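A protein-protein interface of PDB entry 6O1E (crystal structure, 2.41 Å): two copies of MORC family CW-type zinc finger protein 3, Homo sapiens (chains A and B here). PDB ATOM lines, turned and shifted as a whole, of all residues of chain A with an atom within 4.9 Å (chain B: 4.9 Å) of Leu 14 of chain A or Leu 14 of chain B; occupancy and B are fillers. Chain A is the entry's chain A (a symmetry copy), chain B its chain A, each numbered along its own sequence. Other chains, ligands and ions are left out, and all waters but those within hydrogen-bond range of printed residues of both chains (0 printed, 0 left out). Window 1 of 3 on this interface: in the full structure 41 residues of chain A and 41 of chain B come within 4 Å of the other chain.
O of Leu 14 of chain B lies within hydrogen-bond range of N of Val 143 of chain B, 3.0 Å away.
O of Leu 14 of chain A is in hydrogen-bond range of N of Val 143 of chain A (3.0 Å).
Of chain B, only Leu 14 and Phe 83 come within 4 Å of Leu 14 of chain A.
Of chain A, only Leu 14 and Phe 83 come within 4 Å of Leu 14 of chain B.
Printed residues of chain B within 4 Å of Phe 83 of chain A: Ser 12 (3.9 Å), Ala 13 (3.1 Å), Leu 14 (3.8 Å), Cys 15 (2.9 Å) and Phe 18 (3.7 Å).
Printed residues of chain A within 4 Å of Phe 83 of chain B: Ser 12, Ala 13, Leu 14, Cys 15 and Phe 18.
Printed residues of chain B within 4 Å of Phe 18 of chain A: Phe 18 and Phe 83.
Of the printed residues of chain A, Phe 85 of chain B touches Ala 13 (3.8 Å), Cys 15 (3.6 Å) and Glu 141 (3.8 Å).
Printed residues of chain A within 4 Å of Cys 15 of chain B: Phe 83 and Phe 85.
The nearest residue of chain A that does not touch Leu 14 of chain B is Phe 85 of chain A (4.3 Å).
Among the printed residues, pairs that only touch across the chains: Leu 14 of chain A with Leu 14 of chain B, Cys 15 of chain A with Phe 85 of chain B, Phe 85 of chain A with Cys 15 of chain B, Phe 83 of chain A with Phe 18 of chain B, Phe 18 of chain A with Phe 83 of chain B, Phe 83 of chain A with Leu 14 of chain B, Leu 14 of chain A with Phe 83 of chain B, Glu 141 of chain A with Phe 85 of chain B, Phe 85 of chain A with Glu 141 of chain B, Phe 85 of chain A with Ala 13 of chain B, Ala 13 of chain A with Phe 85 of chain B, Phe 18 of chain A with Phe 18 of chain B, Phe 83 of chain A with Ser 12 of chain B and Ser 12 of chain A with Phe 83 of chain B.
Of the 11 printed residues of chain A, 9 touch a printed residue of chain B.
Of the 11 printed residues of chain B, 9 touch a printed residue of chain A.
Printed residues of chain B that touch a printed residue of chain A: Ser 12, Ala 13, Leu 14, Cys 15, Phe 18, Phe 83, Phe 85, Glu 141 and Val 143.
Hydrophobic or aromatic side chains of chain B within 4 Å of the printed part of chain A: Ala 13, Leu 14, Phe 18, Phe 83, Phe 85 and Val 143.
Among the printed residues, 20 pairs touch across the chains.
Among the printed residues, no Asp or Glu carboxylate lies within 4 Å of a Lys or Arg side-chain nitrogen of the other chain.
The backbone NH (N) of Ser 12 of chain B lies within hydrogen-bond range of the backbone carbonyl oxygen (O) of Val 143 of chain A (2.8 Å).
O of Ala 13 of chain B lies within hydrogen-bond range of N of Phe 83 of chain A, at 3.1 Å.
The backbone carbonyl oxygen (O) of Phe 83 of chain A is in hydrogen-bond range of the backbone NH (N) of Cys 15 of chain B.
O of Ala 13 of chain A lies within hydrogen-bond range of N of Phe 83 of chain B (3.1 Å).
O of Phe 83 of chain B sits at hydrogen-bond distance from N of Cys 15 of chain A (2.9 Å).
The backbone carbonyl oxygen (O) of Val 143 of chain B is in hydrogen-bond range of the backbone NH (N) of Ser 12 of chain A (2.8 Å).
Ala 13 of chain A touches Phe 83 of chain B, and with the chains exchanged Phe 83 of chain A touches Ala 13 of chain B.
Leu 14 of chain A touches Phe 83 of chain B, and with the chains exchanged Phe 83 of chain A touches Leu 14 of chain B.
Phe 18 of chain A touches its own counterpart, Phe 18 of chain B.
Phe 85 of chain A touches Glu 141 of chain B, and with the chains exchanged Glu 141 of chain A touches Phe 85 of chain B.
Positions printed for both chains: 12, 13, 14, 15, 16, 18, 83, 85, 141, 142 and 143.
Of the 20 pairs that touch across the chains among the printed residues, 20 have their exchanged pair printed and touching as well.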
ATOM      1  N   SER A  12      17.248 -12.699 -34.840  1.00  0.00           N
ATOM      2  CA  SER A  12      18.199 -13.771 -34.567  1.00  0.00           C
ATOM      3  C   SER A  12      18.105 -14.162 -33.099  1.00  0.00           C
ATOM      4  O   SER A  12      18.107 -13.297 -32.217  1.00  0.00           O
ATOM      5  CB  SER A  12      19.617 -13.329 -34.911  1.00  0.00           C
ATOM      6  OG  SER A  12      20.495 -14.436 -34.910  1.00  0.00           O
ATOM      7  N   ALA A  13      17.980 -15.461 -32.835  1.00  0.00           N
ATOM      8  CA  ALA A  13      17.748 -15.928 -31.475  1.00  0.00           C
ATOM      9  C   ALA A  13      19.066 -16.219 -30.760  1.00  0.00           C
ATOM     10  O   ALA A  13      20.120 -16.415 -31.378  1.00  0.00           O
ATOM     11  CB  ALA A  13      16.874 -17.185 -31.467  1.00  0.00           C
ATOM     12  N   LEU A  14      18.984 -16.284 -29.436  1.00  0.00           N
ATOM     13  CA  LEU A  14      20.159 -16.537 -28.607  1.00  0.00           C
ATOM     14  C   LEU A  14      19.834 -17.623 -27.577  1.00  0.00           C
ATOM     15  O   LEU A  14      19.102 -17.385 -26.615  1.00  0.00           O
ATOM     16  CB  LEU A  14      20.638 -15.229 -27.983  1.00  0.00           C
ATOM     17  CG  LEU A  14      21.913 -15.351 -27.170  1.00  0.00           C
ATOM     18  CD1 LEU A  14      22.974 -14.454 -27.771  1.00  0.00           C
ATOM     19  CD2 LEU A  14      21.630 -14.908 -25.759  1.00  0.00           C
ATOM     20  N   CYS A  15      20.377 -18.869 -27.814  1.00  0.00           N
ATOM     21  CA  CYS A  15      20.154 -20.072 -27.008  1.00  0.00           C
ATOM     22  C   CYS A  15      21.040 -20.039 -25.763  1.00  0.00           C
ATOM     23  O   CYS A  15      22.170 -19.552 -25.818  1.00  0.00           O
ATOM     24  CB  CYS A  15      20.455 -21.337 -27.830  1.00  0.00           C
ATOM     25  SG  CYS A  15      20.546 -22.913 -26.855  1.00  0.00           S
ATOM     26  N   PRO A  16      20.553 -20.517 -24.620  1.00  0.00           N
ATOM     27  CA  PRO A  16      21.368 -20.424 -23.394  1.00  0.00           C
ATOM     28  C   PRO A  16      22.662 -21.225 -23.437  1.00  0.00           C
ATOM     29  O   PRO A  16      23.597 -20.877 -22.704  1.00  0.00           O
ATOM     30  CB  PRO A  16      20.419 -20.925 -22.297  1.00  0.00           C
ATOM     31  CG  PRO A  16      19.235 -21.524 -23.028  1.00  0.00           C
ATOM     32  CD  PRO A  16      19.140 -20.810 -24.322  1.00  0.00           C
ATOM     33  N   PHE A  18      24.739 -20.824 -25.576  1.00  0.00           N
ATOM     34  CA  PHE A  18      25.688 -19.823 -26.030  1.00  0.00           C
ATOM     35  C   PHE A  18      26.326 -19.049 -24.888  1.00  0.00           C
ATOM     36  O   PHE A  18      27.410 -18.491 -25.078  1.00  0.00           O
ATOM     37  CB  PHE A  18      25.026 -18.845 -26.997  1.00  0.00           C
ATOM     38  CG  PHE A  18      26.004 -17.955 -27.695  1.00  0.00           C
ATOM     39  CD1 PHE A  18      26.779 -18.443 -28.740  1.00  0.00           C
ATOM     40  CD2 PHE A  18      26.171 -16.645 -27.297  1.00  0.00           C
ATOM     41  CE1 PHE A  18      27.687 -17.639 -29.369  1.00  0.00           C
ATOM     42  CE2 PHE A  18      27.085 -15.829 -27.923  1.00  0.00           C
ATOM     43  CZ  PHE A  18      27.842 -16.324 -28.960  1.00  0.00           C
ATOM     44  N   PHE A  83      24.393  -8.616 -25.668  1.00  0.00           N
ATOM     45  CA  PHE A  83      25.606  -8.902 -26.421  1.00  0.00           C
ATOM     46  C   PHE A  83      25.846  -7.808 -27.447  1.00  0.00           C
ATOM     47  O   PHE A  83      25.015  -7.592 -28.336  1.00  0.00           O
ATOM     48  CB  PHE A  83      25.510 -10.265 -27.110  1.00  0.00           C
ATOM     49  CG  PHE A  83      25.504 -11.428 -26.154  1.00  0.00           C
ATOM     50  CD1 PHE A  83      26.661 -12.160 -25.927  1.00  0.00           C
ATOM     51  CD2 PHE A  83      24.346 -11.793 -25.489  1.00  0.00           C
ATOM     52  CE1 PHE A  83      26.669 -13.246 -25.039  1.00  0.00           C
ATOM     53  CE2 PHE A  83      24.340 -12.864 -24.597  1.00  0.00           C
ATOM     54  CZ  PHE A  83      25.512 -13.594 -24.372  1.00  0.00           C
ATOM     55  N   PHE A  85      26.490  -4.407 -27.042  1.00  0.00           N
ATOM     56  CA  PHE A  85      26.183  -3.017 -26.716  1.00  0.00           C
ATOM     57  C   PHE A  85      27.383  -2.432 -25.991  1.00  0.00           C
ATOM     58  O   PHE A  85      27.639  -2.763 -24.831  1.00  0.00           O
ATOM     59  CB  PHE A  85      24.920  -2.906 -25.858  1.00  0.00           C
ATOM     60  CG  PHE A  85      23.688  -3.360 -26.569  1.00  0.00           C
ATOM     61  CD1 PHE A  85      23.322  -4.700 -26.557  1.00  0.00           C
ATOM     62  CD2 PHE A  85      22.924  -2.464 -27.294  1.00  0.00           C
ATOM     63  CE1 PHE A  85      22.204  -5.126 -27.241  1.00  0.00           C
ATOM     64  CE2 PHE A  85      21.815  -2.886 -27.968  1.00  0.00           C
ATOM     65  CZ  PHE A  85      21.451  -4.219 -27.954  1.00  0.00           C
ATOM     66  N   GLU A 141      14.452 -21.787 -24.083  1.00  0.00           N
ATOM     67  CA  GLU A 141      15.165 -21.855 -25.350  1.00  0.00           C
ATOM     68  C   GLU A 141      15.695 -20.494 -25.793  1.00  0.00           C
ATOM     69  O   GLU A 141      16.342 -20.402 -26.845  1.00  0.00           O
ATOM     70  CB  GLU A 141      14.291 -22.481 -26.448  1.00  0.00           C
ATOM     71  CG  GLU A 141      12.884 -21.906 -26.638  1.00  0.00           C
ATOM     72  CD  GLU A 141      11.941 -22.921 -27.301  1.00  0.00           C
ATOM     73  OE1 GLU A 141      12.344 -24.106 -27.412  1.00  0.00           O
ATOM     74  OE2 GLU A 141      10.821 -22.539 -27.723  1.00  0.00           O
ATOM     75  N   HIS A 142      15.445 -19.445 -25.013  1.00  0.00           N
ATOM     76  CA  HIS A 142      16.067 -18.144 -25.199  1.00  0.00           C
ATOM     77  C   HIS A 142      16.709 -17.715 -23.886  1.00  0.00           C
ATOM     78  O   HIS A 142      16.327 -18.177 -22.804  1.00  0.00           O
ATOM     79  CB  HIS A 142      15.061 -17.089 -25.662  1.00  0.00           C
ATOM     80  CG  HIS A 142      14.395 -17.424 -26.959  1.00  0.00           C
ATOM     81  ND1 HIS A 142      15.027 -17.285 -28.177  1.00  0.00           N
ATOM     82  CD2 HIS A 142      13.151 -17.885 -27.231  1.00  0.00           C
ATOM     83  CE1 HIS A 142      14.203 -17.655 -29.142  1.00  0.00           C
ATOM     84  NE2 HIS A 142      13.057 -18.018 -28.596  1.00  0.00           N
ATOM     85  N   VAL A 143      17.716 -16.851 -23.990  1.00  0.00           N
ATOM     86  CA  VAL A 143      18.292 -16.232 -22.802  1.00  0.00           C
ATOM     87  C   VAL A 143      17.398 -15.071 -22.375  1.00  0.00           C
ATOM     88  O   VAL A 143      17.110 -14.166 -23.166  1.00  0.00           O
ATOM     89  CB  VAL A 143      19.731 -15.757 -23.052  1.00  0.00           C
ATOM     90  CG1 VAL A 143      20.250 -14.980 -21.831  1.00  0.00           C
ATOM     91  CG2 VAL A 143      20.634 -16.935 -23.360  1.00  0.00           C
ATOM     92  N   SER B  12      17.395 -11.363 -23.451  1.00  0.00           N
ATOM     93  CA  SER B  12      18.710 -10.778 -23.696  1.00  0.00           C
ATOM     94  C   SER B  12      18.820 -10.392 -25.164  1.00  0.00           C
ATOM     95  O   SER B  12      18.487 -11.185 -26.050  1.00  0.00           O
ATOM     96  CB  SER B  12      19.811 -11.765 -23.320  1.00  0.00           C
ATOM     97  OG  SER B  12      21.067 -11.117 -23.296  1.00  0.00           O
ATOM     98  N   ALA B  13      19.248  -9.158 -25.424  1.00  0.00           N
ATOM     99  CA  ALA B  13      19.261  -8.644 -26.787  1.00  0.00           C
ATOM    100  C   ALA B  13      20.597  -8.925 -27.469  1.00  0.00           C
ATOM    101  O   ALA B  13      21.625  -9.177 -26.825  1.00  0.00           O
ATOM    102  CB  ALA B  13      18.983  -7.138 -26.808  1.00  0.00           C
ATOM    103  N   LEU B  14      20.582  -8.839 -28.794  1.00  0.00           N
ATOM    104  CA  LEU B  14      21.775  -9.097 -29.593  1.00  0.00           C
ATOM    105  C   LEU B  14      21.951  -7.978 -30.625  1.00  0.00           C
ATOM    106  O   LEU B  14      21.209  -7.899 -31.606  1.00  0.00           O
ATOM    107  CB  LEU B  14      21.687 -10.488 -30.213  1.00  0.00           C
ATOM    108  CG  LEU B  14      22.919 -10.907 -30.995  1.00  0.00           C
ATOM    109  CD1 LEU B  14      23.500 -12.158 -30.374  1.00  0.00           C
ATOM    110  CD2 LEU B  14      22.512 -11.201 -32.414  1.00  0.00           C
ATOM    111  N   CYS B  15      22.953  -7.066 -30.370  1.00  0.00           N
ATOM    112  CA  CYS B  15      23.265  -5.882 -31.174  1.00  0.00           C
ATOM    113  C   CYS B  15      24.087  -6.283 -32.399  1.00  0.00           C
ATOM    114  O   CYS B  15      24.914  -7.192 -32.319  1.00  0.00           O
ATOM    115  CB  CYS B  15      24.041  -4.849 -30.339  1.00  0.00           C
ATOM    116  SG  CYS B  15      24.796  -3.455 -31.303  1.00  0.00           S
ATOM    117  N   PRO B  16      23.867  -5.653 -33.550  1.00  0.00           N
ATOM    118  CA  PRO B  16      24.601  -6.080 -34.756  1.00  0.00           C
ATOM    119  C   PRO B  16      26.109  -5.882 -34.680  1.00  0.00           C
ATOM    120  O   PRO B  16      26.834  -6.588 -35.392  1.00  0.00           O
ATOM    121  CB  PRO B  16      23.968  -5.238 -35.873  1.00  0.00           C
ATOM    122  CG  PRO B  16      23.120  -4.200 -35.167  1.00  0.00           C
ATOM    123  CD  PRO B  16      22.709  -4.805 -33.879  1.00  0.00           C
ATOM    124  N   PHE B  18      27.785  -7.093 -32.494  1.00  0.00           N
ATOM    125  CA  PHE B  18      28.226  -8.394 -32.022  1.00  0.00           C
ATOM    126  C   PHE B  18      28.515  -9.366 -33.154  1.00  0.00           C
ATOM    127  O   PHE B  18      29.268 -10.321 -32.941  1.00  0.00           O
ATOM    128  CB  PHE B  18      27.197  -9.006 -31.077  1.00  0.00           C
ATOM    129  CG  PHE B  18      27.705 -10.217 -30.360  1.00  0.00           C
ATOM    130  CD1 PHE B  18      28.588 -10.086 -29.295  1.00  0.00           C
ATOM    131  CD2 PHE B  18      27.327 -11.482 -30.761  1.00  0.00           C
ATOM    132  CE1 PHE B  18      29.068 -11.190 -28.649  1.00  0.00           C
ATOM    133  CE2 PHE B  18      27.809 -12.598 -30.118  1.00  0.00           C
ATOM    134  CZ  PHE B  18      28.677 -12.455 -29.060  1.00  0.00           C
ATOM    135  N   PHE B  83      22.439 -18.074 -32.472  1.00  0.00           N
ATOM    136  CA  PHE B  83      23.643 -18.309 -31.689  1.00  0.00           C
ATOM    137  C   PHE B  83      23.387 -19.399 -30.663  1.00  0.00           C
ATOM    138  O   PHE B  83      22.520 -19.250 -29.796  1.00  0.00           O
ATOM    139  CB  PHE B  83      24.100 -17.024 -30.996  1.00  0.00           C
ATOM    140  CG  PHE B  83      24.598 -15.966 -31.946  1.00  0.00           C
ATOM    141  CD1 PHE B  83      25.958 -15.777 -32.141  1.00  0.00           C
ATOM    142  CD2 PHE B  83      23.708 -15.160 -32.636  1.00  0.00           C
ATOM    143  CE1 PHE B  83      26.434 -14.795 -33.024  1.00  0.00           C
ATOM    144  CE2 PHE B  83      24.165 -14.186 -33.522  1.00  0.00           C
ATOM    145  CZ  PHE B  83      25.539 -14.005 -33.716  1.00  0.00           C
ATOM    146  N   PHE B  85      22.583 -22.766 -31.071  1.00  0.00           N
ATOM    147  CA  PHE B  85      21.737 -23.908 -31.411  1.00  0.00           C
ATOM    148  C   PHE B  85      22.606 -24.938 -32.110  1.00  0.00           C
ATOM    149  O   PHE B  85      23.003 -24.748 -33.262  1.00  0.00           O
ATOM    150  CB  PHE B  85      20.562 -23.492 -32.299  1.00  0.00           C
ATOM    151  CG  PHE B  85      19.610 -22.568 -31.615  1.00  0.00           C
ATOM    152  CD1 PHE B  85      19.828 -21.196 -31.629  1.00  0.00           C
ATOM    153  CD2 PHE B  85      18.527 -23.065 -30.912  1.00  0.00           C
ATOM    154  CE1 PHE B  85      18.969 -20.344 -30.969  1.00  0.00           C
ATOM    155  CE2 PHE B  85      17.675 -22.220 -30.262  1.00  0.00           C
ATOM    156  CZ  PHE B  85      17.894 -20.856 -30.278  1.00  0.00           C
ATOM    157  N   GLU B 141      18.846  -1.984 -34.224  1.00  0.00           N
ATOM    158  CA  GLU B 141      19.494  -2.210 -32.940  1.00  0.00           C
ATOM    159  C   GLU B 141      19.405  -3.666 -32.492  1.00  0.00           C
ATOM    160  O   GLU B 141      19.932  -4.011 -31.426  1.00  0.00           O
ATOM    161  CB  GLU B 141      18.929  -1.274 -31.860  1.00  0.00           C
ATOM    162  CG  GLU B 141      17.406  -1.218 -31.706  1.00  0.00           C
ATOM    163  CD  GLU B 141      16.951   0.099 -31.060  1.00  0.00           C
ATOM    164  OE1 GLU B 141      17.803   1.013 -30.934  1.00  0.00           O
ATOM    165  OE2 GLU B 141      15.763   0.215 -30.667  1.00  0.00           O
ATOM    166  N   HIS B 142      18.764  -4.523 -33.283  1.00  0.00           N
ATOM    167  CA  HIS B 142      18.791  -5.963 -33.089  1.00  0.00           C
ATOM    168  C   HIS B 142      19.230  -6.626 -34.388  1.00  0.00           C
ATOM    169  O   HIS B 142      19.097  -6.054 -35.477  1.00  0.00           O
ATOM    170  CB  HIS B 142      17.428  -6.509 -32.655  1.00  0.00           C
ATOM    171  CG  HIS B 142      16.929  -5.922 -31.373  1.00  0.00           C
ATOM    172  ND1 HIS B 142      17.419  -6.303 -30.141  1.00  0.00           N
ATOM    173  CD2 HIS B 142      15.979  -4.989 -31.128  1.00  0.00           C
ATOM    174  CE1 HIS B 142      16.798  -5.622 -29.194  1.00  0.00           C
ATOM    175  NE2 HIS B 142      15.917  -4.822 -29.765  1.00  0.00           N
ATOM    176  N   VAL B 143      19.789  -7.827 -34.265  1.00  0.00           N
ATOM    177  CA  VAL B 143      20.086  -8.635 -35.443  1.00  0.00           C
ATOM    178  C   VAL B 143      18.803  -9.326 -35.896  1.00  0.00           C
ATOM    179  O   VAL B 143      18.150 -10.029 -35.117  1.00  0.00           O
ATOM    180  CB  VAL B 143      21.195  -9.659 -35.161  1.00  0.00           C
ATOM    181  CG1 VAL B 143      21.376 -10.587 -36.374  1.00  0.00           C
ATOM    182  CG2 VAL B 143      22.495  -8.956 -34.826  1.00  0.00           C
